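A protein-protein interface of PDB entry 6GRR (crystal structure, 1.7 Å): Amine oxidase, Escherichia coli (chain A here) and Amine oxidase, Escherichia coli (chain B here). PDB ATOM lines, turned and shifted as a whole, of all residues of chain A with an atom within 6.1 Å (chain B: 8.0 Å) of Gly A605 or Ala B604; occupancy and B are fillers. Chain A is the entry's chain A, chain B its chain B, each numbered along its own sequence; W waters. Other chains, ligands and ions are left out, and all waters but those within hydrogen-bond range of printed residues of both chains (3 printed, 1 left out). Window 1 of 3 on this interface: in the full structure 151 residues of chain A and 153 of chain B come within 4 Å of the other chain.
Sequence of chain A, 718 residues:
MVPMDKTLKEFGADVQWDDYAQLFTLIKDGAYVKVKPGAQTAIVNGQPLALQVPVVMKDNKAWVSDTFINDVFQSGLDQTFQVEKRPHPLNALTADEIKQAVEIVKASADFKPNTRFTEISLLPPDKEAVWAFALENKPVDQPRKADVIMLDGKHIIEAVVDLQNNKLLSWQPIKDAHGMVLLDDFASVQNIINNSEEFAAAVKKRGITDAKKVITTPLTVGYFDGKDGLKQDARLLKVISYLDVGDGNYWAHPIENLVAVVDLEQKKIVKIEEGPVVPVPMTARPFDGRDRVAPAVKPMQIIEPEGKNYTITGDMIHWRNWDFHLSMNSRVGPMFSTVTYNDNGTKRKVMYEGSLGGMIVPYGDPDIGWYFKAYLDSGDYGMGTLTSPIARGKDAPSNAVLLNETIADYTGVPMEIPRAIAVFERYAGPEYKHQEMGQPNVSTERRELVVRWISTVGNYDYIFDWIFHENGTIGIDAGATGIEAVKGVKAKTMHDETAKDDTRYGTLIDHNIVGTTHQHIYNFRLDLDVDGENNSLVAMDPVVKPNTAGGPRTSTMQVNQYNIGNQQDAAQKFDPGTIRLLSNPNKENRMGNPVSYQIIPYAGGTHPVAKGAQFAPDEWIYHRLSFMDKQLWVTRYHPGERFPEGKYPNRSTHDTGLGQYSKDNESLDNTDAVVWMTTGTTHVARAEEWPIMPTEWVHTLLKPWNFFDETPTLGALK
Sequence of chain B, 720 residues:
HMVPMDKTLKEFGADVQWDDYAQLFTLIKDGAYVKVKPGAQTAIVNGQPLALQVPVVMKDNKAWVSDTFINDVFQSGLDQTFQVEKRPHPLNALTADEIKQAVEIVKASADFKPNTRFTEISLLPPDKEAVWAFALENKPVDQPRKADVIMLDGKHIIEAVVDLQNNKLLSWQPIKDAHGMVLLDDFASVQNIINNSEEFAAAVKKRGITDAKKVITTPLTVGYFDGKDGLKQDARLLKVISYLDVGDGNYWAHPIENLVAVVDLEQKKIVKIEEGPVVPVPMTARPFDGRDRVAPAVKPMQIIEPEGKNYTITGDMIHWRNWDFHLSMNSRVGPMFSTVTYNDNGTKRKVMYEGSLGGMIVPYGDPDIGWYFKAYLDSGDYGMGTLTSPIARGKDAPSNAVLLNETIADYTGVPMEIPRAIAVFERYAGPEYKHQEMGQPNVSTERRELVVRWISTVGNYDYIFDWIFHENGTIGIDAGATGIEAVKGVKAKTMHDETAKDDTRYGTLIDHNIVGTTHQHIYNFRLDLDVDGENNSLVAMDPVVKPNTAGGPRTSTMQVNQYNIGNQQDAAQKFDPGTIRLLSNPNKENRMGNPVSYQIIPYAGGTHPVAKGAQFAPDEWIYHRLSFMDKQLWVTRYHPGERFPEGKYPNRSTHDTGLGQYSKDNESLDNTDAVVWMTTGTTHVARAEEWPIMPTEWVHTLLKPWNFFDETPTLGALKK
O of Ala A603 is in hydrogen-bond range of N of Gly B606 (3.2 Å). The backbone carbonyl oxygen (O) of Ala B604 is in hydrogen-bond range of the backbone NH (N) of Gly A605 (3.2 Å). The backbone carbonyl oxygen of Thr A606 lies within hydrogen-bond range of the side-chain amino group of Lys B704, at 2.8 Å. The backbone NH (N) of Val A609 sits at hydrogen-bond distance from the backbone carbonyl oxygen (O) of Pro B577.
The backbone carbonyl oxygen (O) of His A699 lies within hydrogen-bond range of the backbone NH (N) of Ala A603. N of His A699 lies within hydrogen-bond range of O of Gly A604 (3.0 Å). The side-chain hydroxyl (OG1) of Thr A606 sits at hydrogen-bond distance from the backbone NH (N) of Trp A697 (2.9 Å). The backbone NH (N) of Ile B601 lies within hydrogen-bond range of the backbone carbonyl oxygen (O) of Leu B702 (2.9 Å). The backbone carbonyl oxygen of His B700 lies within hydrogen-bond range of the backbone NH of Ala B604 (2.9 Å). The backbone NH (N) of His B700 lies within hydrogen-bond range of the backbone carbonyl oxygen (O) of Gly B605 (2.9 Å).
Among the printed residues, merely in contact across the chains: Tyr A602 with Pro B577, Tyr A602 with Tyr B603, Ala A603 with Gly B605, Gly A604 with Ala B604, Gly A604 with Gly B605, Thr A606 with Leu B702 and His A607 with Lys B704.
Of chain B, only Ala B604 and Gly B605 come within 4 Å of Gly A604. Gly A605 touches just one residue of chain B: Ala B604 (3.2 Å). Of the printed residues of chain A, Pro B577 touches Tyr A602 (3.7 Å) and Val A609 (3.0 Å). Of the printed residues of chain A, Lys B704 touches Thr A606 and His A607.
Of the 20 printed residues of chain B, 7 touch a printed residue of chain A. Printed residues of chain A that touch a printed residue of chain B: Tyr A602, Ala A603, Gly A604, Gly A605, Thr A606, His A607 and Val A609. Hydrophobic or aromatic side chains of chain A within 4 Å of the printed part of chain B: Tyr A602, Ala A603, His A607 and Val A609.
Water W1 bridges the side-chain hydroxyl of Tyr A602 (2.5 Å) and the backbone carbonyl oxygen of Tyr B603 (3.0 Å). Water W2 lies within hydrogen-bond range of the backbone carbonyl oxygen (O) of Ala B604 (2.8 Å) and a ring nitrogen (NE2) of His A699 (3.2 Å). Water W3 lies within hydrogen-bond range of O of Ala A603 (2.9 Å) and NE2 of His B700 (3.3 Å).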
ATOM      1  N   TYR A 602     -20.672 -11.996  19.625  1.00  0.00           N
ATOM      2  CA  TYR A 602     -19.641 -10.967  19.391  1.00  0.00           C
ATOM      3  C   TYR A 602     -19.836  -9.822  20.353  1.00  0.00           C
ATOM      4  O   TYR A 602     -20.689  -8.958  20.128  1.00  0.00           O
ATOM      5  CB  TYR A 602     -19.661 -10.507  17.943  1.00  0.00           C
ATOM      6  CG  TYR A 602     -18.852  -9.261  17.705  1.00  0.00           C
ATOM      7  CD1 TYR A 602     -17.478  -9.229  17.925  1.00  0.00           C
ATOM      8  CD2 TYR A 602     -19.485  -8.095  17.275  1.00  0.00           C
ATOM      9  CE1 TYR A 602     -16.754  -8.065  17.720  1.00  0.00           C
ATOM     10  CE2 TYR A 602     -18.777  -6.934  17.060  1.00  0.00           C
ATOM     11  CZ  TYR A 602     -17.419  -6.919  17.281  1.00  0.00           C
ATOM     12  OH  TYR A 602     -16.775  -5.723  17.042  1.00  0.00           O
ATOM     13  N   ALA A 603     -19.078  -9.846  21.454  1.00  0.00           N
ATOM     14  CA  ALA A 603     -19.061  -8.774  22.446  1.00  0.00           C
ATOM     15  C   ALA A 603     -17.738  -7.976  22.370  1.00  0.00           C
ATOM     16  O   ALA A 603     -17.429  -7.205  23.265  1.00  0.00           O
ATOM     17  CB  ALA A 603     -19.270  -9.351  23.833  1.00  0.00           C
ATOM     18  N   GLY A 604     -17.011  -8.128  21.279  1.00  0.00           N
ATOM     19  CA  GLY A 604     -15.814  -7.313  21.032  1.00  0.00           C
ATOM     20  C   GLY A 604     -14.562  -8.121  20.846  1.00  0.00           C
ATOM     21  O   GLY A 604     -14.554  -9.360  20.874  1.00  0.00           O
ATOM     22  N   GLY A 605     -13.491  -7.383  20.611  1.00  0.00           N
ATOM     23  CA  GLY A 605     -12.204  -7.968  20.448  1.00  0.00           C
ATOM     24  C   GLY A 605     -11.185  -6.912  20.098  1.00  0.00           C
ATOM     25  O   GLY A 605     -11.541  -5.787  19.765  1.00  0.00           O
ATOM     26  N   THR A 606      -9.921  -7.319  20.147  1.00  0.00           N
ATOM     27  CA  THR A 606      -8.802  -6.432  20.007  1.00  0.00           C
ATOM     28  C   THR A 606      -8.119  -6.545  18.657  1.00  0.00           C
ATOM     29  O   THR A 606      -7.298  -5.704  18.349  1.00  0.00           O
ATOM     30  CB  THR A 606      -7.811  -6.677  21.161  1.00  0.00           C
ATOM     31  OG1 THR A 606      -7.322  -8.020  21.090  1.00  0.00           O
ATOM     32  CG2 THR A 606      -8.505  -6.482  22.515  1.00  0.00           C
ATOM     33  N   HIS A 607      -8.442  -7.578  17.871  1.00  0.00           N
ATOM     34  CA  HIS A 607      -8.084  -7.669  16.451  1.00  0.00           C
ATOM     35  C   HIS A 607      -9.321  -7.387  15.583  1.00  0.00           C
ATOM     36  O   HIS A 607     -10.462  -7.444  16.050  1.00  0.00           O
ATOM     37  CB  HIS A 607      -7.555  -9.071  16.099  1.00  0.00           C
ATOM     38  CG  HIS A 607      -6.057  -9.242  16.191  1.00  0.00           C
ATOM     39  ND1 HIS A 607      -5.469 -10.489  16.277  1.00  0.00           N
ATOM     40  CD2 HIS A 607      -5.034  -8.353  16.141  1.00  0.00           C
ATOM     41  CE1 HIS A 607      -4.155 -10.354  16.295  1.00  0.00           C
ATOM     42  NE2 HIS A 607      -3.863  -9.069  16.237  1.00  0.00           N
ATOM     43  N   VAL A 609     -12.522  -7.946  13.381  1.00  0.00           N
ATOM     44  CA  VAL A 609     -13.519  -9.010  13.519  1.00  0.00           C
ATOM     45  C   VAL A 609     -13.748  -9.636  12.156  1.00  0.00           C
ATOM     46  O   VAL A 609     -13.740  -8.954  11.130  1.00  0.00           O
ATOM     47  CB  VAL A 609     -14.869  -8.489  14.029  1.00  0.00           C
ATOM     48  CG1 VAL A 609     -15.822  -9.644  14.379  1.00  0.00           C
ATOM     49  CG2 VAL A 609     -14.672  -7.591  15.236  1.00  0.00           C
ATOM     50  N   THR A 681     -11.536 -13.554  14.317  1.00  0.00           N
ATOM     51  CA  THR A 681     -10.791 -12.366  13.942  1.00  0.00           C
ATOM     52  C   THR A 681     -10.149 -12.579  12.583  1.00  0.00           C
ATOM     53  O   THR A 681      -9.950 -13.710  12.174  1.00  0.00           O
ATOM     54  CB  THR A 681      -9.685 -12.078  14.965  1.00  0.00           C
ATOM     55  OG1 THR A 681      -8.730 -13.148  14.953  1.00  0.00           O
ATOM     56  CG2 THR A 681     -10.285 -11.938  16.368  1.00  0.00           C
ATOM     57  N   TRP A 697      -7.476 -10.551  22.452  1.00  0.00           N
ATOM     58  CA  TRP A 697      -8.669 -11.176  23.040  1.00  0.00           C
ATOM     59  C   TRP A 697      -9.911 -10.937  22.198  1.00  0.00           C
ATOM     60  O   TRP A 697     -10.051  -9.888  21.574  1.00  0.00           O
ATOM     61  CB  TRP A 697      -8.908 -10.594  24.432  1.00  0.00           C
ATOM     62  CG  TRP A 697      -7.908 -11.032  25.483  1.00  0.00           C
ATOM     63  CD1 TRP A 697      -6.798 -10.364  25.894  1.00  0.00           C
ATOM     64  CD2 TRP A 697      -7.981 -12.220  26.280  1.00  0.00           C
ATOM     65  NE1 TRP A 697      -6.155 -11.067  26.885  1.00  0.00           N
ATOM     66  CE2 TRP A 697      -6.868 -12.206  27.153  1.00  0.00           C
ATOM     67  CE3 TRP A 697      -8.883 -13.287  26.348  1.00  0.00           C
ATOM     68  CZ2 TRP A 697      -6.627 -13.225  28.065  1.00  0.00           C
ATOM     69  CZ3 TRP A 697      -8.647 -14.303  27.245  1.00  0.00           C
ATOM     70  CH2 TRP A 697      -7.524 -14.271  28.096  1.00  0.00           C
ATOM     71  N   VAL A 698     -10.826 -11.908  22.244  1.00  0.00           N
ATOM     72  CA  VAL A 698     -12.205 -11.748  21.768  1.00  0.00           C
ATOM     73  C   VAL A 698     -13.146 -12.126  22.921  1.00  0.00           C
ATOM     74  O   VAL A 698     -12.775 -12.920  23.771  1.00  0.00           O
ATOM     75  CB  VAL A 698     -12.543 -12.589  20.515  1.00  0.00           C
ATOM     76  CG1 VAL A 698     -11.633 -12.230  19.357  1.00  0.00           C
ATOM     77  CG2 VAL A 698     -12.442 -14.074  20.780  1.00  0.00           C
ATOM     78  N   HIS A 699     -14.328 -11.521  22.926  1.00  0.00           N
ATOM     79  CA  HIS A 699     -15.280 -11.613  24.038  1.00  0.00           C
ATOM     80  C   HIS A 699     -16.627 -12.079  23.534  1.00  0.00           C
ATOM     81  O   HIS A 699     -17.106 -11.641  22.492  1.00  0.00           O
ATOM     82  CB  HIS A 699     -15.478 -10.260  24.740  1.00  0.00           C
ATOM     83  CG  HIS A 699     -14.215  -9.502  24.959  1.00  0.00           C
ATOM     84  ND1 HIS A 699     -13.292  -9.863  25.914  1.00  0.00           N
ATOM     85  CD2 HIS A 699     -13.700  -8.425  24.321  1.00  0.00           C
ATOM     86  CE1 HIS A 699     -12.276  -9.019  25.877  1.00  0.00           C
ATOM     87  NE2 HIS A 699     -12.490  -8.148  24.910  1.00  0.00           N
ATOM     88  N   GLY B 476      -6.472   2.044  25.757  1.00  0.00           N
ATOM     89  CA  GLY B 476      -7.895   1.748  25.799  1.00  0.00           C
ATOM     90  C   GLY B 476      -8.702   2.898  26.342  1.00  0.00           C
ATOM     91  O   GLY B 476      -8.249   3.611  27.219  1.00  0.00           O
ATOM     92  N   ILE B 477      -9.931   3.076  25.858  1.00  0.00           N
ATOM     93  CA  ILE B 477     -10.879   4.013  26.472  1.00  0.00           C
ATOM     94  C   ILE B 477     -12.194   3.260  26.590  1.00  0.00           C
ATOM     95  O   ILE B 477     -12.800   2.871  25.574  1.00  0.00           O
ATOM     96  CB  ILE B 477     -11.069   5.327  25.694  1.00  0.00           C
ATOM     97  CG1 ILE B 477      -9.718   5.949  25.326  1.00  0.00           C
ATOM     98  CG2 ILE B 477     -11.928   6.312  26.493  1.00  0.00           C
ATOM     99  CD1 ILE B 477      -9.821   7.040  24.278  1.00  0.00           C
ATOM    100  N   ASP B 478     -12.597   3.016  27.826  1.00  0.00           N
ATOM    101  CA  ASP B 478     -13.838   2.291  28.114  1.00  0.00           C
ATOM    102  C   ASP B 478     -14.808   3.199  28.829  1.00  0.00           C
ATOM    103  O   ASP B 478     -14.393   4.015  29.673  1.00  0.00           O
ATOM    104  CB  ASP B 478     -13.557   1.069  28.966  1.00  0.00           C
ATOM    105  CG  ASP B 478     -12.780  -0.007  28.231  1.00  0.00           C
ATOM    106  OD1 ASP B 478     -12.405   0.136  27.044  1.00  0.00           O
ATOM    107  OD2 ASP B 478     -12.505  -1.022  28.889  1.00  0.00           O
ATOM    108  N   PHE B 575     -18.000   2.873  11.113  1.00  0.00           N
ATOM    109  CA  PHE B 575     -16.856   1.987  11.360  1.00  0.00           C
ATOM    110  C   PHE B 575     -17.272   0.537  11.207  1.00  0.00           C
ATOM    111  O   PHE B 575     -18.146   0.047  11.943  1.00  0.00           O
ATOM    112  CB  PHE B 575     -16.273   2.203  12.748  1.00  0.00           C
ATOM    113  CG  PHE B 575     -15.094   1.310  13.046  1.00  0.00           C
ATOM    114  CD1 PHE B 575     -13.904   1.445  12.333  1.00  0.00           C
ATOM    115  CD2 PHE B 575     -15.178   0.321  14.030  1.00  0.00           C
ATOM    116  CE1 PHE B 575     -12.813   0.619  12.593  1.00  0.00           C
ATOM    117  CE2 PHE B 575     -14.091  -0.503  14.295  1.00  0.00           C
ATOM    118  CZ  PHE B 575     -12.907  -0.360  13.578  1.00  0.00           C
ATOM    119  N   PRO B 577     -15.898  -2.952  11.910  1.00  0.00           N
ATOM    120  CA  PRO B 577     -14.836  -3.507  12.751  1.00  0.00           C
ATOM    121  C   PRO B 577     -14.022  -4.625  12.102  1.00  0.00           C
ATOM    122  O   PRO B 577     -13.091  -5.120  12.728  1.00  0.00           O
ATOM    123  CB  PRO B 577     -15.604  -4.013  13.988  1.00  0.00           C
ATOM    124  CG  PRO B 577     -16.933  -4.383  13.444  1.00  0.00           C
ATOM    125  CD  PRO B 577     -17.234  -3.388  12.368  1.00  0.00           C
ATOM    126  N   ILE B 601      -9.772   2.131  16.725  1.00  0.00           N
ATOM    127  CA  ILE B 601     -10.852   1.158  16.871  1.00  0.00           C
ATOM    128  C   ILE B 601     -11.977   1.769  17.720  1.00  0.00           C
ATOM    129  O   ILE B 601     -11.986   1.644  18.961  1.00  0.00           O
ATOM    130  CB  ILE B 601     -10.379  -0.173  17.490  1.00  0.00           C
ATOM    131  CG1 ILE B 601      -9.178  -0.714  16.712  1.00  0.00           C
ATOM    132  CG2 ILE B 601     -11.538  -1.184  17.535  1.00  0.00           C
ATOM    133  CD1 ILE B 601      -8.559  -1.984  17.207  1.00  0.00           C
ATOM    134  N   PRO B 602     -12.941   2.438  17.062  1.00  0.00           N
ATOM    135  CA  PRO B 602     -14.034   3.055  17.817  1.00  0.00           C
ATOM    136  C   PRO B 602     -14.996   2.052  18.391  1.00  0.00           C
ATOM    137  O   PRO B 602     -15.798   2.422  19.222  1.00  0.00           O
ATOM    138  CB  PRO B 602     -14.786   3.904  16.769  1.00  0.00           C
ATOM    139  CG  PRO B 602     -13.907   3.957  15.580  1.00  0.00           C
ATOM    140  CD  PRO B 602     -12.953   2.812  15.633  1.00  0.00           C
ATOM    141  N   TYR B 603     -14.997   0.833  17.870  1.00  0.00           N
ATOM    142  CA  TYR B 603     -15.841  -0.222  18.442  1.00  0.00           C
ATOM    143  C   TYR B 603     -15.018  -1.463  18.680  1.00  0.00           C
ATOM    144  O   TYR B 603     -14.711  -2.209  17.732  1.00  0.00           O
ATOM    145  CB  TYR B 603     -17.068  -0.579  17.565  1.00  0.00           C
ATOM    146  CG  TYR B 603     -17.951  -1.554  18.345  1.00  0.00           C
ATOM    147  CD1 TYR B 603     -18.540  -1.149  19.536  1.00  0.00           C
ATOM    148  CD2 TYR B 603     -18.129  -2.887  17.946  1.00  0.00           C
ATOM    149  CE1 TYR B 603     -19.310  -2.008  20.301  1.00  0.00           C
ATOM    150  CE2 TYR B 603     -18.914  -3.759  18.714  1.00  0.00           C
ATOM    151  CZ  TYR B 603     -19.495  -3.305  19.889  1.00  0.00           C
ATOM    152  OH  TYR B 603     -20.270  -4.118  20.706  1.00  0.00           O
ATOM    153  N   ALA B 604     -14.647  -1.674  19.944  1.00  0.00           N
ATOM    154  CA  ALA B 604     -13.928  -2.866  20.369  1.00  0.00           C
ATOM    155  C   ALA B 604     -14.784  -3.717  21.295  1.00  0.00           C
ATOM    156  O   ALA B 604     -14.269  -4.634  21.954  1.00  0.00           O
ATOM    157  CB  ALA B 604     -12.628  -2.502  21.050  1.00  0.00           C
ATOM    158  N   GLY B 605     -16.074  -3.426  21.319  1.00  0.00           N
ATOM    159  CA  GLY B 605     -17.031  -4.296  22.002  1.00  0.00           C
ATOM    160  C   GLY B 605     -17.852  -3.598  23.030  1.00  0.00           C
ATOM    161  O   GLY B 605     -17.688  -2.423  23.289  1.00  0.00           O
ATOM    162  N   GLY B 606     -18.783  -4.346  23.597  1.00  0.00           N
ATOM    163  CA  GLY B 606     -19.577  -3.845  24.687  1.00  0.00           C
ATOM    164  C   GLY B 606     -20.569  -4.900  25.123  1.00  0.00           C
ATOM    165  O   GLY B 606     -20.733  -5.939  24.467  1.00  0.00           O
ATOM    166  N   VAL B 610     -25.134  -2.896  20.251  1.00  0.00           N
ATOM    167  CA  VAL B 610     -24.422  -1.779  19.674  1.00  0.00           C
ATOM    168  C   VAL B 610     -25.318  -0.895  18.811  1.00  0.00           C
ATOM    169  O   VAL B 610     -26.208  -1.362  18.100  1.00  0.00           O
ATOM    170  CB  VAL B 610     -23.168  -2.221  18.887  1.00  0.00           C
ATOM    171  CG1 VAL B 610     -23.522  -2.872  17.560  1.00  0.00           C
ATOM    172  CG2 VAL B 610     -22.254  -1.020  18.627  1.00  0.00           C
ATOM    173  N   THR B 680     -19.018   6.000  19.947  1.00  0.00           N
ATOM    174  CA  THR B 680     -19.435   4.656  20.261  1.00  0.00           C
ATOM    175  C   THR B 680     -20.702   4.713  21.091  1.00  0.00           C
ATOM    176  O   THR B 680     -20.870   5.541  21.990  1.00  0.00           O
ATOM    177  CB  THR B 680     -18.319   3.831  20.948  1.00  0.00           C
ATOM    178  OG1 THR B 680     -18.799   2.507  21.204  1.00  0.00           O
ATOM    179  CG2 THR B 680     -17.851   4.446  22.238  1.00  0.00           C
ATOM    180  N   TRP B 698     -20.634  -1.925  29.963  1.00  0.00           N
ATOM    181  CA  TRP B 698     -19.401  -1.312  29.403  1.00  0.00           C
ATOM    182  C   TRP B 698     -19.343  -1.337  27.878  1.00  0.00           C
ATOM    183  O   TRP B 698     -19.842  -2.265  27.259  1.00  0.00           O
ATOM    184  CB  TRP B 698     -18.188  -2.082  29.916  1.00  0.00           C
ATOM    185  CG  TRP B 698     -17.895  -1.875  31.385  1.00  0.00           C
ATOM    186  CD1 TRP B 698     -18.271  -2.667  32.421  1.00  0.00           C
ATOM    187  CD2 TRP B 698     -17.117  -0.808  31.952  1.00  0.00           C
ATOM    188  NE1 TRP B 698     -17.774  -2.169  33.608  1.00  0.00           N
ATOM    189  CE2 TRP B 698     -17.076  -1.017  33.351  1.00  0.00           C
ATOM    190  CE3 TRP B 698     -16.482   0.308  31.413  1.00  0.00           C
ATOM    191  CZ2 TRP B 698     -16.413  -0.162  34.222  1.00  0.00           C
ATOM    192  CZ3 TRP B 698     -15.778   1.171  32.291  1.00  0.00           C
ATOM    193  CH2 TRP B 698     -15.758   0.917  33.677  1.00  0.00           C
ATOM    194  N   VAL B 699     -18.707  -0.319  27.294  1.00  0.00           N
ATOM    195  CA  VAL B 699     -18.287  -0.331  25.899  1.00  0.00           C
ATOM    196  C   VAL B 699     -16.789  -0.033  25.867  1.00  0.00           C
ATOM    197  O   VAL B 699     -16.277   0.652  26.768  1.00  0.00           O
ATOM    198  CB  VAL B 699     -19.044   0.680  25.001  1.00  0.00           C
ATOM    199  CG1 VAL B 699     -20.521   0.339  24.964  1.00  0.00           C
ATOM    200  CG2 VAL B 699     -18.850   2.116  25.468  1.00  0.00           C
ATOM    201  N   HIS B 700     -16.119  -0.579  24.865  1.00  0.00           N
ATOM    202  CA  HIS B 700     -14.643  -0.521  24.775  1.00  0.00           C
ATOM    203  C   HIS B 700     -14.227   0.065  23.453  1.00  0.00           C
ATOM    204  O   HIS B 700     -14.849  -0.216  22.426  1.00  0.00           O
ATOM    205  CB  HIS B 700     -14.002  -1.918  24.908  1.00  0.00           C
ATOM    206  CG  HIS B 700     -14.642  -2.790  25.947  1.00  0.00           C
ATOM    207  ND1 HIS B 700     -14.424  -2.623  27.300  1.00  0.00           N
ATOM    208  CD2 HIS B 700     -15.475  -3.856  25.825  1.00  0.00           C
ATOM    209  CE1 HIS B 700     -15.129  -3.521  27.965  1.00  0.00           C
ATOM    210  NE2 HIS B 700     -15.779  -4.277  27.097  1.00  0.00           N
ATOM    211  N   THR B 701     -13.161   0.868  23.488  1.00  0.00           N
ATOM    212  CA  THR B 701     -12.518   1.395  22.302  1.00  0.00           C
ATOM    213  C   THR B 701     -11.022   1.214  22.500  1.00  0.00           C
ATOM    214  O   THR B 701     -10.548   1.055  23.637  1.00  0.00           O
ATOM    215  CB  THR B 701     -12.809   2.906  22.057  1.00  0.00           C
ATOM    216  OG1 THR B 701     -12.088   3.710  22.996  1.00  0.00           O
ATOM    217  CG2 THR B 701     -14.288   3.249  22.160  1.00  0.00           C
ATOM    218  N   LEU B 702     -10.274   1.235  21.392  1.00  0.00           N
ATOM    219  CA  LEU B 702      -8.827   1.004  21.415  1.00  0.00           C
ATOM    220  C   LEU B 702      -8.073   1.826  20.404  1.00  0.00           C
ATOM    221  O   LEU B 702      -8.560   2.055  19.314  1.00  0.00           O
ATOM    222  CB  LEU B 702      -8.502  -0.442  21.090  1.00  0.00           C
ATOM    223  CG  LEU B 702      -8.601  -1.542  22.119  1.00  0.00           C
ATOM    224  CD1 LEU B 702      -8.235  -2.862  21.444  1.00  0.00           C
ATOM    225  CD2 LEU B 702      -7.711  -1.327  23.342  1.00  0.00           C
ATOM    226  N   LEU B 703      -6.848   2.196  20.777  1.00  0.00           N
ATOM    227  CA  LEU B 703      -5.852   2.785  19.905  1.00  0.00           C
ATOM    228  C   LEU B 703      -4.590   1.922  20.018  1.00  0.00           C
ATOM    229  O   LEU B 703      -4.038   1.793  21.115  1.00  0.00           O
ATOM    230  CB  LEU B 703      -5.549   4.215  20.341  1.00  0.00           C
ATOM    231  CG  LEU B 703      -6.750   5.123  20.579  1.00  0.00           C
ATOM    232  CD1 LEU B 703      -6.324   6.393  21.300  1.00  0.00           C
ATOM    233  CD2 LEU B 703      -7.427   5.460  19.257  1.00  0.00           C
ATOM    234  N   LYS B 704      -4.143   1.304  18.927  1.00  0.00           N
ATOM    235  CA  LYS B 704      -3.071   0.322  18.995  1.00  0.00           C
ATOM    236  C   LYS B 704      -1.921   0.805  18.128  1.00  0.00           C
ATOM    237  O   LYS B 704      -2.173   1.188  16.985  1.00  0.00           O
ATOM    238  CB  LYS B 704      -3.496  -1.051  18.487  1.00  0.00           C
ATOM    239  CG  LYS B 704      -4.673  -1.708  19.215  1.00  0.00           C
ATOM    240  CD  LYS B 704      -5.100  -2.993  18.522  1.00  0.00           C
ATOM    241  CE  LYS B 704      -4.124  -4.124  18.783  1.00  0.00           C
ATOM    242  NZ  LYS B 704      -4.532  -5.405  18.158  1.00  0.00           N
HETATM  243  O   HOH W   1     -14.419  -5.176  17.697  1.00  0.00           O
HETATM  244  O   HOH W   2     -12.137  -5.277  23.589  1.00  0.00           O
HETATM  245  O   HOH W   3     -17.488  -6.900  26.119  1.00  0.00           O
